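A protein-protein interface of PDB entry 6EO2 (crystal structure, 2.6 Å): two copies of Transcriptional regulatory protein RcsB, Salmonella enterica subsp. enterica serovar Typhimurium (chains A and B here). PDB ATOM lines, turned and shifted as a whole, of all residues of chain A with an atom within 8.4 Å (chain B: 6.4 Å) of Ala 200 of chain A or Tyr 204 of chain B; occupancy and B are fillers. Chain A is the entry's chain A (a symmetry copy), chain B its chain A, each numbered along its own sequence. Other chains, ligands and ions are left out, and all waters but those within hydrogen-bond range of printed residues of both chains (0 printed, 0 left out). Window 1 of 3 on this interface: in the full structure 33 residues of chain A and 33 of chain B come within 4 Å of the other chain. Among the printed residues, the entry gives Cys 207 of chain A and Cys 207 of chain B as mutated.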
ATOM      1  N   PHE A 162      29.833  -3.657  -4.215  1.00  0.00           N
ATOM      2  CA  PHE A 162      30.371  -2.352  -3.858  1.00  0.00           C
ATOM      3  C   PHE A 162      29.252  -1.464  -3.308  1.00  0.00           C
ATOM      4  O   PHE A 162      29.385  -0.893  -2.231  1.00  0.00           O
ATOM      5  CB  PHE A 162      31.049  -1.672  -5.043  1.00  0.00           C
ATOM      6  CG  PHE A 162      31.952  -0.544  -4.641  1.00  0.00           C
ATOM      7  CD1 PHE A 162      33.143  -0.803  -3.975  1.00  0.00           C
ATOM      8  CD2 PHE A 162      31.616   0.776  -4.925  1.00  0.00           C
ATOM      9  CE1 PHE A 162      33.984   0.233  -3.599  1.00  0.00           C
ATOM     10  CE2 PHE A 162      32.451   1.817  -4.551  1.00  0.00           C
ATOM     11  CZ  PHE A 162      33.637   1.546  -3.886  1.00  0.00           C
ATOM     12  N   MET A 190      33.248   0.402 -14.478  1.00  0.00           N
ATOM     13  CA  MET A 190      33.226   1.849 -14.349  1.00  0.00           C
ATOM     14  C   MET A 190      33.462   2.515 -15.706  1.00  0.00           C
ATOM     15  O   MET A 190      32.872   3.546 -16.005  1.00  0.00           O
ATOM     16  CB  MET A 190      34.284   2.308 -13.344  1.00  0.00           C
ATOM     17  CG  MET A 190      34.044   1.809 -11.935  1.00  0.00           C
ATOM     18  SD  MET A 190      34.993   2.711 -10.713  1.00  0.00           S
ATOM     19  CE  MET A 190      36.661   2.393 -11.264  1.00  0.00           C
ATOM     20  N   LEU A 193      30.225   2.436 -17.766  1.00  0.00           N
ATOM     21  CA  LEU A 193      29.168   3.311 -17.268  1.00  0.00           C
ATOM     22  C   LEU A 193      29.479   4.794 -17.435  1.00  0.00           C
ATOM     23  O   LEU A 193      28.576   5.625 -17.386  1.00  0.00           O
ATOM     24  CB  LEU A 193      28.897   3.004 -15.794  1.00  0.00           C
ATOM     25  CG  LEU A 193      28.295   1.620 -15.553  1.00  0.00           C
ATOM     26  CD1 LEU A 193      28.429   1.236 -14.094  1.00  0.00           C
ATOM     27  CD2 LEU A 193      26.840   1.577 -15.986  1.00  0.00           C
ATOM     28  N   GLY A 194      30.751   5.120 -17.626  1.00  0.00           N
ATOM     29  CA  GLY A 194      31.179   6.501 -17.777  1.00  0.00           C
ATOM     30  C   GLY A 194      31.468   7.160 -16.443  1.00  0.00           C
ATOM     31  O   GLY A 194      31.249   8.361 -16.287  1.00  0.00           O
ATOM     32  N   VAL A 195      31.975   6.383 -15.483  1.00  0.00           N
ATOM     33  CA  VAL A 195      32.290   6.908 -14.153  1.00  0.00           C
ATOM     34  C   VAL A 195      33.790   6.783 -13.869  1.00  0.00           C
ATOM     35  O   VAL A 195      34.422   5.803 -14.263  1.00  0.00           O
ATOM     36  CB  VAL A 195      31.440   6.248 -13.045  1.00  0.00           C
ATOM     37  CG1 VAL A 195      29.959   6.458 -13.325  1.00  0.00           C
ATOM     38  CG2 VAL A 195      31.753   4.764 -12.896  1.00  0.00           C
ATOM     39  N   GLU A 196      34.346   7.802 -13.215  1.00  0.00           N
ATOM     40  CA  GLU A 196      35.787   7.922 -13.010  1.00  0.00           C
ATOM     41  C   GLU A 196      36.190   7.796 -11.555  1.00  0.00           C
ATOM     42  O   GLU A 196      37.372   7.789 -11.257  1.00  0.00           O
ATOM     43  CB  GLU A 196      36.287   9.281 -13.504  1.00  0.00           C
ATOM     44  CG  GLU A 196      36.019   9.553 -14.969  1.00  0.00           C
ATOM     45  CD  GLU A 196      36.453  10.948 -15.413  1.00  0.00           C
ATOM     46  OE1 GLU A 196      36.156  11.947 -14.708  1.00  0.00           O
ATOM     47  OE2 GLU A 196      37.088  11.044 -16.489  1.00  0.00           O
ATOM     48  N   ASN A 197      35.225   7.733 -10.645  1.00  0.00           N
ATOM     49  CA  ASN A 197      35.531   7.556  -9.238  1.00  0.00           C
ATOM     50  C   ASN A 197      34.378   6.900  -8.470  1.00  0.00           C
ATOM     51  O   ASN A 197      33.244   6.803  -8.968  1.00  0.00           O
ATOM     52  CB  ASN A 197      35.915   8.898  -8.617  1.00  0.00           C
ATOM     53  CG  ASN A 197      34.748   9.859  -8.540  1.00  0.00           C
ATOM     54  OD1 ASN A 197      33.812   9.644  -7.771  1.00  0.00           O
ATOM     55  ND2 ASN A 197      34.797  10.925  -9.328  1.00  0.00           N
ATOM     56  N   ASP A 198      34.679   6.474  -7.247  1.00  0.00           N
ATOM     57  CA  ASP A 198      33.751   5.661  -6.459  1.00  0.00           C
ATOM     58  C   ASP A 198      32.508   6.418  -6.034  1.00  0.00           C
ATOM     59  O   ASP A 198      31.414   5.859  -6.022  1.00  0.00           O
ATOM     60  CB  ASP A 198      34.446   5.089  -5.225  1.00  0.00           C
ATOM     61  CG  ASP A 198      35.546   4.113  -5.582  1.00  0.00           C
ATOM     62  OD1 ASP A 198      35.718   3.814  -6.785  1.00  0.00           O
ATOM     63  OD2 ASP A 198      36.240   3.644  -4.657  1.00  0.00           O
ATOM     64  N   ILE A 199      32.671   7.685  -5.686  1.00  0.00           N
ATOM     65  CA  ILE A 199      31.534   8.493  -5.260  1.00  0.00           C
ATOM     66  C   ILE A 199      30.595   8.764  -6.434  1.00  0.00           C
ATOM     67  O   ILE A 199      29.379   8.735  -6.272  1.00  0.00           O
ATOM     68  CB  ILE A 199      32.005   9.789  -4.570  1.00  0.00           C
ATOM     69  CG1 ILE A 199      32.546   9.439  -3.171  1.00  0.00           C
ATOM     70  CG2 ILE A 199      30.871  10.801  -4.475  1.00  0.00           C
ATOM     71  CD1 ILE A 199      33.533  10.441  -2.606  1.00  0.00           C
ATOM     72  N   ALA A 200      31.161   9.005  -7.612  1.00  0.00           N
ATOM     73  CA  ALA A 200      30.368   9.124  -8.831  1.00  0.00           C
ATOM     74  C   ALA A 200      29.643   7.812  -9.128  1.00  0.00           C
ATOM     75  O   ALA A 200      28.466   7.807  -9.489  1.00  0.00           O
ATOM     76  CB  ALA A 200      31.252   9.516 -10.005  1.00  0.00           C
ATOM     77  N   LEU A 201      30.361   6.704  -8.968  1.00  0.00           N
ATOM     78  CA  LEU A 201      29.798   5.372  -9.165  1.00  0.00           C
ATOM     79  C   LEU A 201      28.641   5.077  -8.204  1.00  0.00           C
ATOM     80  O   LEU A 201      27.589   4.569  -8.606  1.00  0.00           O
ATOM     81  CB  LEU A 201      30.903   4.327  -8.993  1.00  0.00           C
ATOM     82  CG  LEU A 201      30.520   2.851  -9.026  1.00  0.00           C
ATOM     83  CD1 LEU A 201      29.968   2.460 -10.388  1.00  0.00           C
ATOM     84  CD2 LEU A 201      31.730   2.002  -8.670  1.00  0.00           C
ATOM     85  N   LEU A 202      28.835   5.393  -6.932  1.00  0.00           N
ATOM     86  CA  LEU A 202      27.815   5.107  -5.931  1.00  0.00           C
ATOM     87  C   LEU A 202      26.592   6.007  -6.121  1.00  0.00           C
ATOM     88  O   LEU A 202      25.456   5.553  -5.970  1.00  0.00           O
ATOM     89  CB  LEU A 202      28.397   5.230  -4.522  1.00  0.00           C
ATOM     90  CG  LEU A 202      29.405   4.133  -4.169  1.00  0.00           C
ATOM     91  CD1 LEU A 202      30.080   4.424  -2.834  1.00  0.00           C
ATOM     92  CD2 LEU A 202      28.749   2.764  -4.147  1.00  0.00           C
ATOM     93  N   ASN A 203      26.827   7.271  -6.471  1.00  0.00           N
ATOM     94  CA  ASN A 203      25.744   8.155  -6.910  1.00  0.00           C
ATOM     95  C   ASN A 203      24.992   7.548  -8.092  1.00  0.00           C
ATOM     96  O   ASN A 203      23.780   7.377  -8.039  1.00  0.00           O
ATOM     97  CB  ASN A 203      26.284   9.536  -7.286  1.00  0.00           C
ATOM     98  CG  ASN A 203      26.713  10.347  -6.075  1.00  0.00           C
ATOM     99  OD1 ASN A 203      27.249  11.454  -6.210  1.00  0.00           O
ATOM    100  ND2 ASN A 203      26.486   9.796  -4.880  1.00  0.00           N
ATOM    101  N   TYR A 204      25.732   7.196  -9.140  1.00  0.00           N
ATOM    102  CA  TYR A 204      25.157   6.581 -10.332  1.00  0.00           C
ATOM    103  C   TYR A 204      24.222   5.422  -9.990  1.00  0.00           C
ATOM    104  O   TYR A 204      23.087   5.386 -10.453  1.00  0.00           O
ATOM    105  CB  TYR A 204      26.270   6.090 -11.281  1.00  0.00           C
ATOM    106  CG  TYR A 204      25.815   5.847 -12.714  1.00  0.00           C
ATOM    107  CD1 TYR A 204      25.235   4.633 -13.094  1.00  0.00           C
ATOM    108  CD2 TYR A 204      25.966   6.836 -13.690  1.00  0.00           C
ATOM    109  CE1 TYR A 204      24.815   4.416 -14.401  1.00  0.00           C
ATOM    110  CE2 TYR A 204      25.552   6.627 -15.001  1.00  0.00           C
ATOM    111  CZ  TYR A 204      24.977   5.420 -15.353  1.00  0.00           C
ATOM    112  OH  TYR A 204      24.569   5.219 -16.654  1.00  0.00           O
ATOM    113  N   LEU A 205      24.702   4.484  -9.178  1.00  0.00           N
ATOM    114  CA  LEU A 205      23.986   3.229  -8.947  1.00  0.00           C
ATOM    115  C   LEU A 205      22.707   3.402  -8.133  1.00  0.00           C
ATOM    116  O   LEU A 205      21.763   2.623  -8.292  1.00  0.00           O
ATOM    117  CB  LEU A 205      24.900   2.204  -8.265  1.00  0.00           C
ATOM    118  CG  LEU A 205      26.079   1.679  -9.097  1.00  0.00           C
ATOM    119  CD1 LEU A 205      27.150   1.058  -8.205  1.00  0.00           C
ATOM    120  CD2 LEU A 205      25.608   0.689 -10.153  1.00  0.00           C
ATOM    121  N   SER A 206      22.664   4.423  -7.279  1.00  0.00           N
ATOM    122  CA  SER A 206      21.514   4.627  -6.391  1.00  0.00           C
ATOM    123  C   SER A 206      20.221   5.037  -7.116  1.00  0.00           C
ATOM    124  O   SER A 206      19.168   5.108  -6.493  1.00  0.00           O
ATOM    125  CB  SER A 206      21.854   5.658  -5.314  1.00  0.00           C
ATOM    126  OG  SER A 206      21.962   6.955  -5.871  1.00  0.00           O
ATOM    127  N   CYS A 207      20.304   5.331  -8.411  1.00  0.00           N
ATOM    128  CA  CYS A 207      19.113   5.505  -9.254  1.00  0.00           C
ATOM    129  C   CYS A 207      19.251   4.604 -10.470  1.00  0.00           C
ATOM    130  O   CYS A 207      19.394   5.073 -11.599  1.00  0.00           O
ATOM    131  CB  CYS A 207      18.945   6.966  -9.670  1.00  0.00           C
ATOM    132  SG  CYS A 207      20.495   7.760 -10.149  1.00  0.00           S
ATOM    133  N   GLY B 144      26.533  18.372  -1.840  1.00  0.00           N
ATOM    134  CA  GLY B 144      25.431  17.769  -2.549  1.00  0.00           C
ATOM    135  C   GLY B 144      25.880  16.446  -3.107  1.00  0.00           C
ATOM    136  O   GLY B 144      25.281  15.917  -4.029  1.00  0.00           O
ATOM    137  N   GLY B 145      26.935  15.896  -2.535  1.00  0.00           N
ATOM    138  CA  GLY B 145      27.478  14.653  -3.030  1.00  0.00           C
ATOM    139  C   GLY B 145      28.365  14.791  -4.253  1.00  0.00           C
ATOM    140  O   GLY B 145      28.795  13.779  -4.779  1.00  0.00           O
ATOM    141  N   TYR B 146      28.657  16.009  -4.715  1.00  0.00           N
ATOM    142  CA  TYR B 146      29.564  16.138  -5.855  1.00  0.00           C
ATOM    143  C   TYR B 146      30.902  15.594  -5.437  1.00  0.00           C
ATOM    144  O   TYR B 146      31.579  14.928  -6.197  1.00  0.00           O
ATOM    145  CB  TYR B 146      29.877  17.588  -6.255  1.00  0.00           C
ATOM    146  CG  TYR B 146      28.761  18.569  -6.429  1.00  0.00           C
ATOM    147  CD1 TYR B 146      27.446  18.199  -6.310  1.00  0.00           C
ATOM    148  CD2 TYR B 146      29.049  19.888  -6.718  1.00  0.00           C
ATOM    149  CE1 TYR B 146      26.438  19.122  -6.466  1.00  0.00           C
ATOM    150  CE2 TYR B 146      28.055  20.821  -6.874  1.00  0.00           C
ATOM    151  CZ  TYR B 146      26.746  20.433  -6.749  1.00  0.00           C
ATOM    152  OH  TYR B 146      25.741  21.363  -6.909  1.00  0.00           O
ATOM    153  N   LEU B 193      32.279  15.946 -11.633  1.00  0.00           N
ATOM    154  CA  LEU B 193      31.220  15.006 -11.279  1.00  0.00           C
ATOM    155  C   LEU B 193      31.639  13.545 -11.406  1.00  0.00           C
ATOM    156  O   LEU B 193      31.000  12.667 -10.833  1.00  0.00           O
ATOM    157  CB  LEU B 193      29.987  15.267 -12.146  1.00  0.00           C
ATOM    158  CG  LEU B 193      29.314  16.611 -11.873  1.00  0.00           C
ATOM    159  CD1 LEU B 193      28.379  16.970 -13.008  1.00  0.00           C
ATOM    160  CD2 LEU B 193      28.566  16.585 -10.551  1.00  0.00           C
ATOM    161  N   GLY B 194      32.703  13.292 -12.157  1.00  0.00           N
ATOM    162  CA  GLY B 194      33.189  11.940 -12.374  1.00  0.00           C
ATOM    163  C   GLY B 194      32.507  11.268 -13.550  1.00  0.00           C
ATOM    164  O   GLY B 194      32.306  10.054 -13.536  1.00  0.00           O
ATOM    165  N   VAL B 195      32.165  12.049 -14.576  1.00  0.00           N
ATOM    166  CA  VAL B 195      31.498  11.515 -15.765  1.00  0.00           C
ATOM    167  C   VAL B 195      32.372  11.713 -17.006  1.00  0.00           C
ATOM    168  O   VAL B 195      33.047  12.733 -17.138  1.00  0.00           O
ATOM    169  CB  VAL B 195      30.083  12.104 -15.959  1.00  0.00           C
ATOM    170  CG1 VAL B 195      29.224  11.822 -14.736  1.00  0.00           C
ATOM    171  CG2 VAL B 195      30.126  13.599 -16.251  1.00  0.00           C
ATOM    172  N   ILE B 199      25.944  10.577 -22.145  1.00  0.00           N
ATOM    173  CA  ILE B 199      24.875   9.701 -21.682  1.00  0.00           C
ATOM    174  C   ILE B 199      25.028   9.405 -20.191  1.00  0.00           C
ATOM    175  O   ILE B 199      24.040   9.366 -19.464  1.00  0.00           O
ATOM    176  CB  ILE B 199      24.804   8.418 -22.533  1.00  0.00           C
ATOM    177  CG1 ILE B 199      24.204   8.766 -23.909  1.00  0.00           C
ATOM    178  CG2 ILE B 199      23.977   7.345 -21.838  1.00  0.00           C
ATOM    179  CD1 ILE B 199      24.576   7.805 -25.021  1.00  0.00           C
ATOM    180  N   ALA B 200      26.264   9.221 -19.740  1.00  0.00           N
ATOM    181  CA  ALA B 200      26.545   9.085 -18.314  1.00  0.00           C
ATOM    182  C   ALA B 200      26.160  10.363 -17.569  1.00  0.00           C
ATOM    183  O   ALA B 200      25.564  10.313 -16.494  1.00  0.00           O
ATOM    184  CB  ALA B 200      28.016   8.767 -18.090  1.00  0.00           C
ATOM    185  N   LEU B 201      26.506  11.504 -18.158  1.00  0.00           N
ATOM    186  CA  LEU B 201      26.168  12.809 -17.598  1.00  0.00           C
ATOM    187  C   LEU B 201      24.653  13.020 -17.482  1.00  0.00           C
ATOM    188  O   LEU B 201      24.149  13.480 -16.452  1.00  0.00           O
ATOM    189  CB  LEU B 201      26.787  13.906 -18.465  1.00  0.00           C
ATOM    190  CG  LEU B 201      26.456  15.359 -18.144  1.00  0.00           C
ATOM    191  CD1 LEU B 201      26.982  15.751 -16.773  1.00  0.00           C
ATOM    192  CD2 LEU B 201      27.033  16.265 -19.222  1.00  0.00           C
ATOM    193  N   LEU B 202      23.928  12.688 -18.540  1.00  0.00           N
ATOM    194  CA  LEU B 202      22.486  12.897 -18.548  1.00  0.00           C
ATOM    195  C   LEU B 202      21.786  11.938 -17.583  1.00  0.00           C
ATOM    196  O   LEU B 202      20.841  12.327 -16.894  1.00  0.00           O
ATOM    197  CB  LEU B 202      21.934  12.775 -19.969  1.00  0.00           C
ATOM    198  CG  LEU B 202      22.356  13.916 -20.899  1.00  0.00           C
ATOM    199  CD1 LEU B 202      21.931  13.633 -22.334  1.00  0.00           C
ATOM    200  CD2 LEU B 202      21.796  15.248 -20.430  1.00  0.00           C
ATOM    201  N   ASN B 203      22.265  10.696 -17.521  1.00  0.00           N
ATOM    202  CA  ASN B 203      21.838   9.765 -16.473  1.00  0.00           C
ATOM    203  C   ASN B 203      22.085  10.356 -15.086  1.00  0.00           C
ATOM    204  O   ASN B 203      21.167  10.462 -14.281  1.00  0.00           O
ATOM    205  CB  ASN B 203      22.560   8.423 -16.605  1.00  0.00           C
ATOM    206  CG  ASN B 203      22.073   7.611 -17.793  1.00  0.00           C
ATOM    207  OD1 ASN B 203      22.611   6.536 -18.091  1.00  0.00           O
ATOM    208  ND2 ASN B 203      21.052   8.123 -18.485  1.00  0.00           N
ATOM    209  N   TYR B 204      23.324  10.770 -14.837  1.00  0.00           N
ATOM    210  CA  TYR B 204      23.704  11.378 -13.566  1.00  0.00           C
ATOM    211  C   TYR B 204      22.733  12.478 -13.140  1.00  0.00           C
ATOM    212  O   TYR B 204      22.236  12.464 -12.019  1.00  0.00           O
ATOM    213  CB  TYR B 204      25.136  11.948 -13.644  1.00  0.00           C
ATOM    214  CG  TYR B 204      25.788  12.197 -12.290  1.00  0.00           C
ATOM    215  CD1 TYR B 204      25.571  13.387 -11.589  1.00  0.00           C
ATOM    216  CD2 TYR B 204      26.627  11.240 -11.713  1.00  0.00           C
ATOM    217  CE1 TYR B 204      26.163  13.609 -10.351  1.00  0.00           C
ATOM    218  CE2 TYR B 204      27.227  11.454 -10.477  1.00  0.00           C
ATOM    219  CZ  TYR B 204      26.993  12.636  -9.799  1.00  0.00           C
ATOM    220  OH  TYR B 204      27.590  12.843  -8.575  1.00  0.00           O
ATOM    221  N   LEU B 205      22.466  13.423 -14.037  1.00  0.00           N
ATOM    222  CA  LEU B 205      21.724  14.633 -13.680  1.00  0.00           C
ATOM    223  C   LEU B 205      20.249  14.375 -13.384  1.00  0.00           C
ATOM    224  O   LEU B 205      19.639  15.106 -12.598  1.00  0.00           O
ATOM    225  CB  LEU B 205      21.853  15.691 -14.783  1.00  0.00           C
ATOM    226  CG  LEU B 205      23.249  16.295 -14.990  1.00  0.00           C
ATOM    227  CD1 LEU B 205      23.368  16.953 -16.362  1.00  0.00           C
ATOM    228  CD2 LEU B 205      23.590  17.282 -13.882  1.00  0.00           C
ATOM    229  N   SER B 206      19.681  13.335 -13.992  1.00  0.00           N
ATOM    230  CA  SER B 206      18.250  13.050 -13.839  1.00  0.00           C
ATOM    231  C   SER B 206      17.845  12.588 -12.429  1.00  0.00           C
ATOM    232  O   SER B 206      16.660  12.448 -12.150  1.00  0.00           O
ATOM    233  CB  SER B 206      17.803  12.017 -14.873  1.00  0.00           C
ATOM    234  OG  SER B 206      18.335  10.740 -14.574  1.00  0.00           O
ATOM    235  N   CYS B 207      18.817  12.327 -11.560  1.00  0.00           N
ATOM    236  CA  CYS B 207      18.555  12.108 -10.131  1.00  0.00           C
ATOM    237  C   CYS B 207      19.449  13.041  -9.331  1.00  0.00           C
ATOM    238  O   CYS B 207      20.359  12.604  -8.627  1.00  0.00           O
ATOM    239  CB  CYS B 207      18.800  10.648  -9.746  1.00  0.00           C
ATOM    240  SG  CYS B 207      20.289   9.950 -10.492  1.00  0.00           S
ATOM    241  N   VAL B 208      19.169  14.334  -9.477  1.00  0.00           N
ATOM    242  CA  VAL B 208      19.950  15.417  -8.882  1.00  0.00           C
ATOM    243  C   VAL B 208      19.483  16.731  -9.511  1.00  0.00           C
ATOM    244  O   VAL B 208      19.823  17.818  -9.044  1.00  0.00           O
ATOM    245  CB  VAL B 208      21.442  15.214  -9.119  1.00  0.00           C
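The backbone carbonyl oxygen (O) of Gly 145 of chain B lies close to the side-chain amide oxygen (OD1) of Asn 203 of chain A (3.1 Å).
The backbone carbonyl oxygen (O) of Gly 194 of chain B sits at hydrogen-bond distance from the backbone NH (N) of Glu 196 of chain A.
OH of Tyr 204 of chain A is in hydrogen-bond range of OD1 of Asn 203 of chain B (2.8 Å).
OD1 of Asn 203 of chain A is in hydrogen-bond range of OH of Tyr 204 of chain B.
SG of Cys 207 of chain B forms a disulfide with SG of Cys 207 of chain A (2.2 Å).
The backbone carbonyl oxygen (O) of Gly 194 of chain B lies close to the backbone carbonyl oxygen (O) of Gly 194 of chain A, 3.4 Å away.
O of Leu 193 of chain A touches CB of Ala 200 of chain B, at 3.3 Å.
CA of Val 195 of chain B touches O of Gly 194 of chain A, 3.2 Å away.
Gly 194 of chain A touches Ala 200 of chain B (O to CB, 3.7 Å).
Glu 196 of chain A touches Val 195 of chain B (OE1 to N, 3.99 Å).
ND2 of Asn 197 of chain A touches CA of Gly 194 of chain B, at 3.6 Å.
O of Gly 145 of chain B touches CG2 of Ile 199 of chain A, at 3.6 Å.
CB of Ala 200 of chain A touches O of Leu 193 of chain B (3.3 Å).
O of Gly 194 of chain B touches CB of Ala 200 of chain A, 3.7 Å away.
Tyr 204 of chain B touches Ala 200 of chain A.
Tyr 204 of chain A touches Ala 200 of chain B.
Of the 17 printed residues of chain A, 10 touch a printed residue of chain B.
Printed residues of chain A that touch a printed residue of chain B: Leu 193, Gly 194, Val 195, Glu 196, Asn 197, Ile 199, Ala 200, Asn 203, Tyr 204 and Cys 207.
Hydrophobic or aromatic side chains of chain A that line the printed part of chain B: Val 195, Ile 199, Ala 200 and Tyr 204.
Among the printed residues, 17 pairs touch across the chains.
ND2 of Asn 203 of chain B sits close to O of Ile 199 of chain B.
O of Asn 203 of chain B lies within hydrogen-bond range of OG of Ser 206 of chain B, at 2.9 Å.
N of Val 195 of chain A lies within hydrogen-bond range of O of Met 190 of chain A (3.0 Å).
N of Ile 199 of chain A is in hydrogen-bond range of OD1 of Asn 197 of chain A.
The backbone carbonyl oxygen (O) of Ile 199 of chain A sits close to the side-chain amide nitrogen (ND2) of Asn 203 of chain A.
O of Asn 203 of chain A lies within hydrogen-bond range of OG of Ser 206 of chain A, 2.9 Å away.
Of chain B, only Leu 193, Gly 194 and Tyr 204 come within 4 Å of Ala 200 of chain A.
Of the printed residues of chain B, Tyr 204 of chain A touches Ala 200 (3.98 Å) and Asn 203 (2.8 Å).
Ser 206 of chain A touches none of the printed residues of chain B.
Of the printed residues of chain B, Cys 207 of chain A touches Cys 207.
Of the printed residues of chain A, Leu 193 of chain B touches Ala 200 (3.3 Å).
Leu 202 of chain B touches none of the printed residues of chain A.
Of chain A, only Ala 200 and Asn 203 come within 4 Å of Tyr 204 of chain B.
Of the printed residues of chain A, Cys 207 of chain B touches Cys 207.
Gly 194 of chain B touches its own counterpart, Gly 194 of chain A.
Gly 194 of chain A touches Ala 200 of chain B, and with the chains exchanged Ala 200 of chain A touches Gly 194 of chain B.
Asn 203 of chain A touches Tyr 204 of chain B, and with the chains exchanged Tyr 204 of chain A touches Asn 203 of chain B.
Cys 207 of chain A touches its own counterpart, Cys 207 of chain B.
Positions printed for both chains: 193, 194, 195, 199, 200, 201, 202, 203, 204, 205, 206 and 207.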
